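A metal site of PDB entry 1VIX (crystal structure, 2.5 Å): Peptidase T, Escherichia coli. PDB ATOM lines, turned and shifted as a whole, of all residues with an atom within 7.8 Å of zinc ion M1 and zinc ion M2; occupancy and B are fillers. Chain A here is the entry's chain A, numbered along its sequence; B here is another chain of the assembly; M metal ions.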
ATOM      1  N   SER A  79     -14.174 -19.009  17.233  1.00  0.00           N
ATOM      2  CA  SER A  79     -13.914 -17.573  17.343  1.00  0.00           C
ATOM      3  C   SER A  79     -14.370 -17.105  18.725  1.00  0.00           C
ATOM      4  O   SER A  79     -15.127 -17.793  19.384  1.00  0.00           O
ATOM      5  CB  SER A  79     -14.631 -16.782  16.239  1.00  0.00           C
ATOM      6  OG  SER A  79     -13.805 -16.641  15.085  1.00  0.00           O
ATOM      7  N   HIS A  80     -13.876 -15.961  19.177  1.00  0.00           N
ATOM      8  CA  HIS A  80     -14.289 -15.465  20.490  1.00  0.00           C
ATOM      9  C   HIS A  80     -15.222 -14.254  20.360  1.00  0.00           C
ATOM     10  O   HIS A  80     -15.084 -13.454  19.422  1.00  0.00           O
ATOM     11  CB  HIS A  80     -13.075 -15.168  21.359  1.00  0.00           C
ATOM     12  CG  HIS A  80     -12.147 -14.132  20.801  1.00  0.00           C
ATOM     13  ND1 HIS A  80     -12.316 -12.789  21.035  1.00  0.00           N
ATOM     14  CD2 HIS A  80     -11.039 -14.240  20.035  1.00  0.00           C
ATOM     15  CE1 HIS A  80     -11.351 -12.109  20.433  1.00  0.00           C
ATOM     16  NE2 HIS A  80     -10.566 -12.975  19.813  1.00  0.00           N
ATOM     17  N   ASP A  82     -15.788 -11.742  22.569  1.00  0.00           N
ATOM     18  CA  ASP A  82     -15.428 -10.545  23.316  1.00  0.00           C
ATOM     19  C   ASP A  82     -14.450  -9.662  22.560  1.00  0.00           C
ATOM     20  O   ASP A  82     -13.733 -10.138  21.676  1.00  0.00           O
ATOM     21  CB  ASP A  82     -14.834 -10.907  24.679  1.00  0.00           C
ATOM     22  CG  ASP A  82     -13.579 -11.733  24.550  1.00  0.00           C
ATOM     23  OD1 ASP A  82     -13.630 -12.773  23.848  1.00  0.00           O
ATOM     24  OD2 ASP A  82     -12.502 -11.442  25.109  1.00  0.00           O
ATOM     25  N   THR A  83     -14.424  -8.374  22.915  1.00  0.00           N
ATOM     26  CA  THR A  83     -13.430  -7.447  22.391  1.00  0.00           C
ATOM     27  C   THR A  83     -12.536  -6.935  23.513  1.00  0.00           C
ATOM     28  O   THR A  83     -12.875  -7.052  24.679  1.00  0.00           O
ATOM     29  CB  THR A  83     -14.096  -6.285  21.621  1.00  0.00           C
ATOM     30  OG1 THR A  83     -15.159  -5.719  22.402  1.00  0.00           O
ATOM     31  CG2 THR A  83     -14.794  -6.806  20.378  1.00  0.00           C
ATOM     32  N   SER A  84     -11.379  -6.364  23.150  1.00  0.00           N
ATOM     33  CA  SER A  84     -10.336  -6.005  24.111  1.00  0.00           C
ATOM     34  C   SER A  84     -10.732  -4.930  25.135  1.00  0.00           C
ATOM     35  O   SER A  84     -11.495  -4.018  24.819  1.00  0.00           O
ATOM     36  CB  SER A  84      -9.071  -5.556  23.378  1.00  0.00           C
ATOM     37  OG  SER A  84      -8.024  -5.320  24.301  1.00  0.00           O
ATOM     38  N   ALA A 141     -13.285  -6.176  14.725  1.00  0.00           N
ATOM     39  CA  ALA A 141     -13.006  -7.149  13.667  1.00  0.00           C
ATOM     40  C   ALA A 141     -12.396  -8.361  14.367  1.00  0.00           C
ATOM     41  O   ALA A 141     -12.678  -9.505  14.031  1.00  0.00           O
ATOM     42  CB  ALA A 141     -12.045  -6.576  12.652  1.00  0.00           C
ATOM     43  N   ASP A 142     -11.568  -8.056  15.364  1.00  0.00           N
ATOM     44  CA  ASP A 142     -11.085  -9.038  16.327  1.00  0.00           C
ATOM     45  C   ASP A 142     -12.116  -9.099  17.445  1.00  0.00           C
ATOM     46  O   ASP A 142     -12.159  -8.214  18.298  1.00  0.00           O
ATOM     47  CB  ASP A 142      -9.740  -8.579  16.884  1.00  0.00           C
ATOM     48  CG  ASP A 142      -9.105  -9.612  17.760  1.00  0.00           C
ATOM     49  OD1 ASP A 142      -7.939  -9.402  18.161  1.00  0.00           O
ATOM     50  OD2 ASP A 142      -9.671 -10.668  18.119  1.00  0.00           O
ATOM     51  N   ASP A 143     -12.973 -10.119  17.455  1.00  0.00           N
ATOM     52  CA  ASP A 143     -12.933 -11.241  16.527  1.00  0.00           C
ATOM     53  C   ASP A 143     -14.316 -11.452  15.929  1.00  0.00           C
ATOM     54  O   ASP A 143     -14.714 -12.572  15.595  1.00  0.00           O
ATOM     55  CB  ASP A 143     -12.463 -12.503  17.264  1.00  0.00           C
ATOM     56  CG  ASP A 143     -12.167 -13.655  16.325  1.00  0.00           C
ATOM     57  OD1 ASP A 143     -12.432 -14.817  16.724  1.00  0.00           O
ATOM     58  OD2 ASP A 143     -11.675 -13.502  15.180  1.00  0.00           O
ATOM     59  N   LYS A 144     -15.063 -10.361  15.794  1.00  0.00           N
ATOM     60  CA  LYS A 144     -16.428 -10.431  15.263  1.00  0.00           C
ATOM     61  C   LYS A 144     -16.446 -10.583  13.735  1.00  0.00           C
ATOM     62  O   LYS A 144     -17.462 -10.968  13.145  1.00  0.00           O
ATOM     63  CB  LYS A 144     -17.233  -9.221  15.720  1.00  0.00           C
ATOM     64  CG  LYS A 144     -17.522  -9.212  17.202  1.00  0.00           C
ATOM     65  CD  LYS A 144     -17.771  -7.795  17.715  1.00  0.00           C
ATOM     66  CE  LYS A 144     -18.377  -7.828  19.098  1.00  0.00           C
ATOM     67  NZ  LYS A 144     -18.522  -6.468  19.690  1.00  0.00           N
ATOM     68  N   GLU A 175     -11.571 -14.609  25.742  1.00  0.00           N
ATOM     69  CA  GLU A 175     -10.292 -14.769  25.080  1.00  0.00           C
ATOM     70  C   GLU A 175      -9.293 -13.643  25.365  1.00  0.00           C
ATOM     71  O   GLU A 175      -8.113 -13.916  25.593  1.00  0.00           O
ATOM     72  CB  GLU A 175     -10.477 -14.925  23.576  1.00  0.00           C
ATOM     73  CG  GLU A 175      -9.272 -15.482  22.839  1.00  0.00           C
ATOM     74  CD  GLU A 175      -8.228 -14.423  22.521  1.00  0.00           C
ATOM     75  OE1 GLU A 175      -8.598 -13.244  22.314  1.00  0.00           O
ATOM     76  OE2 GLU A 175      -7.028 -14.775  22.490  1.00  0.00           O
ATOM     77  N   GLU A 176      -9.762 -12.397  25.356  1.00  0.00           N
ATOM     78  CA  GLU A 176      -8.877 -11.249  25.558  1.00  0.00           C
ATOM     79  C   GLU A 176      -8.417 -11.054  27.010  1.00  0.00           C
ATOM     80  O   GLU A 176      -7.691 -10.103  27.309  1.00  0.00           O
ATOM     81  CB  GLU A 176      -9.509  -9.952  25.041  1.00  0.00           C
ATOM     82  CG  GLU A 176      -9.778  -9.917  23.531  1.00  0.00           C
ATOM     83  CD  GLU A 176      -8.522  -9.726  22.699  1.00  0.00           C
ATOM     84  OE1 GLU A 176      -8.426 -10.394  21.641  1.00  0.00           O
ATOM     85  OE2 GLU A 176      -7.644  -8.910  23.075  1.00  0.00           O
ATOM     86  N   THR A 196      -8.794 -21.681  14.847  1.00  0.00           N
ATOM     87  CA  THR A 196      -9.376 -20.418  15.279  1.00  0.00           C
ATOM     88  C   THR A 196      -9.361 -19.455  14.104  1.00  0.00           C
ATOM     89  O   THR A 196      -8.360 -19.354  13.383  1.00  0.00           O
ATOM     90  CB  THR A 196      -8.639 -19.782  16.481  1.00  0.00           C
ATOM     91  OG1 THR A 196      -7.234 -19.703  16.204  1.00  0.00           O
ATOM     92  CG2 THR A 196      -8.757 -20.666  17.721  1.00  0.00           C
ATOM     93  N   VAL A 197     -10.465 -18.763  13.911  1.00  0.00           N
ATOM     94  CA  VAL A 197     -10.527 -17.729  12.894  1.00  0.00           C
ATOM     95  C   VAL A 197     -10.316 -16.424  13.647  1.00  0.00           C
ATOM     96  O   VAL A 197     -11.258 -15.726  14.000  1.00  0.00           O
ATOM     97  CB  VAL A 197     -11.860 -17.808  12.104  1.00  0.00           C
ATOM     98  CG1 VAL A 197     -11.856 -16.835  10.946  1.00  0.00           C
ATOM     99  CG2 VAL A 197     -12.085 -19.220  11.591  1.00  0.00           C
ATOM    100  N   ASP A 198      -9.039 -16.125  13.905  1.00  0.00           N
ATOM    101  CA  ASP A 198      -8.632 -15.011  14.759  1.00  0.00           C
ATOM    102  C   ASP A 198      -7.262 -14.458  14.356  1.00  0.00           C
ATOM    103  O   ASP A 198      -6.559 -13.852  15.170  1.00  0.00           O
ATOM    104  CB  ASP A 198      -8.622 -15.481  16.219  1.00  0.00           C
ATOM    105  CG  ASP A 198      -8.584 -14.327  17.201  1.00  0.00           C
ATOM    106  OD1 ASP A 198      -9.104 -13.243  16.882  1.00  0.00           O
ATOM    107  OD2 ASP A 198      -8.046 -14.406  18.326  1.00  0.00           O
ATOM    108  N   GLY A 199      -6.896 -14.668  13.087  1.00  0.00           N
ATOM    109  CA  GLY A 199      -5.654 -14.148  12.537  1.00  0.00           C
ATOM    110  C   GLY A 199      -5.856 -12.765  11.954  1.00  0.00           C
ATOM    111  O   GLY A 199      -6.841 -12.089  12.267  1.00  0.00           O
ATOM    112  N   GLY A 357       0.233 -15.876  23.332  1.00  0.00           N
ATOM    113  CA  GLY A 357      -0.615 -17.053  23.410  1.00  0.00           C
ATOM    114  C   GLY A 357      -1.929 -16.898  22.685  1.00  0.00           C
ATOM    115  O   GLY A 357      -2.374 -15.774  22.396  1.00  0.00           O
ATOM    116  N   THR A 358      -2.552 -18.028  22.363  1.00  0.00           N
ATOM    117  CA  THR A 358      -3.905 -18.050  21.820  1.00  0.00           C
ATOM    118  C   THR A 358      -4.728 -19.091  22.571  1.00  0.00           C
ATOM    119  O   THR A 358      -4.172 -19.865  23.358  1.00  0.00           O
ATOM    120  CB  THR A 358      -3.899 -18.377  20.313  1.00  0.00           C
ATOM    121  OG1 THR A 358      -2.860 -19.324  20.036  1.00  0.00           O
ATOM    122  CG2 THR A 358      -3.505 -17.140  19.495  1.00  0.00           C
ATOM    123  N   ASP A 359      -6.031 -19.079  22.329  1.00  0.00           N
ATOM    124  CA  ASP A 359      -6.938 -20.127  22.812  1.00  0.00           C
ATOM    125  C   ASP A 359      -6.522 -21.461  22.221  1.00  0.00           C
ATOM    126  O   ASP A 359      -6.515 -22.479  22.918  1.00  0.00           O
ATOM    127  CB  ASP A 359      -8.363 -19.822  22.393  1.00  0.00           C
ATOM    128  CG  ASP A 359      -9.052 -18.885  23.320  1.00  0.00           C
ATOM    129  OD1 ASP A 359     -10.218 -18.529  23.040  1.00  0.00           O
ATOM    130  OD2 ASP A 359      -8.514 -18.430  24.359  1.00  0.00           O
ATOM    131  N   ASN A 372      -4.147 -21.009  13.851  1.00  0.00           N
ATOM    132  CA  ASN A 372      -4.914 -19.773  13.690  1.00  0.00           C
ATOM    133  C   ASN A 372      -5.040 -19.336  12.227  1.00  0.00           C
ATOM    134  O   ASN A 372      -4.062 -19.368  11.503  1.00  0.00           O
ATOM    135  CB  ASN A 372      -4.301 -18.639  14.520  1.00  0.00           C
ATOM    136  CG  ASN A 372      -5.264 -17.503  14.777  1.00  0.00           C
ATOM    137  OD1 ASN A 372      -6.487 -17.705  14.830  1.00  0.00           O
ATOM    138  ND2 ASN A 372      -4.737 -16.297  14.939  1.00  0.00           N
ATOM    139  N   THR A 375      -8.395 -13.267   9.253  1.00  0.00           N
ATOM    140  CA  THR A 375      -9.696 -12.650   9.362  1.00  0.00           C
ATOM    141  C   THR A 375      -9.855 -11.523   8.323  1.00  0.00           C
ATOM    142  O   THR A 375     -10.968 -11.199   7.895  1.00  0.00           O
ATOM    143  CB  THR A 375      -9.859 -12.116  10.785  1.00  0.00           C
ATOM    144  OG1 THR A 375     -10.545 -13.083  11.578  1.00  0.00           O
ATOM    145  CG2 THR A 375     -10.765 -10.942  10.829  1.00  0.00           C
ATOM    146  N   TYR A 380      -5.336  -4.454  15.579  1.00  0.00           N
ATOM    147  CA  TYR A 380      -6.254  -4.890  16.627  1.00  0.00           C
ATOM    148  C   TYR A 380      -5.977  -4.214  17.966  1.00  0.00           C
ATOM    149  O   TYR A 380      -4.841  -3.830  18.248  1.00  0.00           O
ATOM    150  CB  TYR A 380      -6.195  -6.411  16.758  1.00  0.00           C
ATOM    151  CG  TYR A 380      -6.699  -7.153  15.530  1.00  0.00           C
ATOM    152  CD1 TYR A 380      -6.115  -8.344  15.119  1.00  0.00           C
ATOM    153  CD2 TYR A 380      -7.785  -6.652  14.775  1.00  0.00           C
ATOM    154  CE1 TYR A 380      -6.581  -9.032  13.989  1.00  0.00           C
ATOM    155  CE2 TYR A 380      -8.263  -7.331  13.662  1.00  0.00           C
ATOM    156  CZ  TYR A 380      -7.658  -8.518  13.280  1.00  0.00           C
ATOM    157  OH  TYR A 380      -8.128  -9.198  12.179  1.00  0.00           O
ATOM    158  N   HIS A 381      -7.030  -4.056  18.767  1.00  0.00           N
ATOM    159  CA  HIS A 381      -6.938  -3.510  20.133  1.00  0.00           C
ATOM    160  C   HIS A 381      -6.633  -2.010  20.185  1.00  0.00           C
ATOM    161  O   HIS A 381      -5.728  -1.564  20.904  1.00  0.00           O
ATOM    162  CB  HIS A 381      -5.957  -4.323  21.001  1.00  0.00           C
ATOM    163  CG  HIS A 381      -6.091  -5.806  20.855  1.00  0.00           C
ATOM    164  ND1 HIS A 381      -5.016  -6.667  20.936  1.00  0.00           N
ATOM    165  CD2 HIS A 381      -7.175  -6.590  20.618  1.00  0.00           C
ATOM    166  CE1 HIS A 381      -5.432  -7.903  20.766  1.00  0.00           C
ATOM    167  NE2 HIS A 381      -6.739  -7.883  20.570  1.00  0.00           N
ATOM    168  N   GLU A 385      -8.230   0.240  14.239  1.00  0.00           N
ATOM    169  CA  GLU A 385      -8.634  -1.089  13.765  1.00  0.00           C
ATOM    170  C   GLU A 385      -9.507  -0.984  12.515  1.00  0.00           C
ATOM    171  O   GLU A 385     -10.502  -0.249  12.491  1.00  0.00           O
ATOM    172  CB  GLU A 385      -9.343  -1.875  14.860  1.00  0.00           C
ATOM    173  CG  GLU A 385      -9.311  -3.370  14.603  1.00  0.00           C
ATOM    174  CD  GLU A 385     -10.333  -4.146  15.413  1.00  0.00           C
ATOM    175  OE1 GLU A 385     -10.932  -3.586  16.362  1.00  0.00           O
ATOM    176  OE2 GLU A 385     -10.533  -5.323  15.097  1.00  0.00           O
ATOM    177  N   HIS B 225       1.072  -4.608  24.183  1.00  0.00           N
ATOM    178  CA  HIS B 225       1.275  -6.050  24.276  1.00  0.00           C
ATOM    179  C   HIS B 225       2.738  -6.337  23.933  1.00  0.00           C
ATOM    180  O   HIS B 225       3.187  -5.985  22.840  1.00  0.00           O
ATOM    181  CB  HIS B 225       0.342  -6.797  23.314  1.00  0.00           C
ATOM    182  CG  HIS B 225      -1.072  -6.900  23.782  1.00  0.00           C
ATOM    183  ND1 HIS B 225      -2.133  -7.105  22.921  1.00  0.00           N
ATOM    184  CD2 HIS B 225      -1.611  -6.865  25.032  1.00  0.00           C
ATOM    185  CE1 HIS B 225      -3.260  -7.174  23.609  1.00  0.00           C
ATOM    186  NE2 HIS B 225      -2.968  -7.030  24.896  1.00  0.00           N
HETATM  187 ZN    ZN M   1      -7.225 -10.295  19.989  1.00  0.00          ZN
HETATM  188 ZN    ZN M   2      -8.864 -12.445  18.789  1.00  0.00          ZN
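The side-chain carboxylate (OD2) of Asp 82 lies within hydrogen-bond range of the backbone NH (N) of Glu 176 (2.9 Å). A ring nitrogen (NE2) of His 80 sits close to the side-chain carboxylate (OE1) of Glu 175, 3.2 Å away. N of His 80 sits at hydrogen-bond distance from OD1 of Asp 143, at 3.1 Å. ND1 of His 80 sits at hydrogen-bond distance from O of Asp 82 (3.1 Å). The backbone NH (N) of Asp 142 is in hydrogen-bond range of the side-chain carboxylate (OE2) of Glu 385 (2.9 Å). ND2 of Asn 372 sits at hydrogen-bond distance from O of Asp 198 (3.1 Å). OD2 of Asp 143 lies close to O of Val 197 (2.6 Å). The side-chain hydroxyl of Ser 79 is in hydrogen-bond range of the side-chain carboxylate of Asp 143, at 2.8 Å.
Residues that only touch zinc ion M1: Glu 175. Within 4 Å of zinc ion M1: Asp 142, Glu 175, Glu 176 and His 381. The nearest printed residue that does not touch zinc ion M1 is His 80 (4.3 Å).
Asp 143 touches zinc ion M2 (CB to ZN, 3.9 Å). Glu 175 touches zinc ion M2. Six residues have an atom within 4 Å of zinc ion M2: His 80, Asp 142, Asp 143, Glu 175, Glu 176 and Asp 198. Along chain A the residues within 4 Å of zinc ion M2 span positions 80 to 198.
Zinc ion M1 is bound by OE1 of Glu 176. The side-chain carboxylate (OD1) of Asp 142 is bound to zinc ion M1 (2.2 Å). A ring nitrogen (NE2) of His 381 binds zinc ion M1 (2.5 Å).
Zinc ion M2 is bound by a ring nitrogen (NE2) of His 80 (2.1 Å), the side-chain carboxylate (OD2) of Asp 142 (2.1 Å), the side-chain carboxylate (OD1) of Asp 198 (2.1 Å) and the side-chain carboxylate (OD2) of Asp 198 (2.2 Å).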
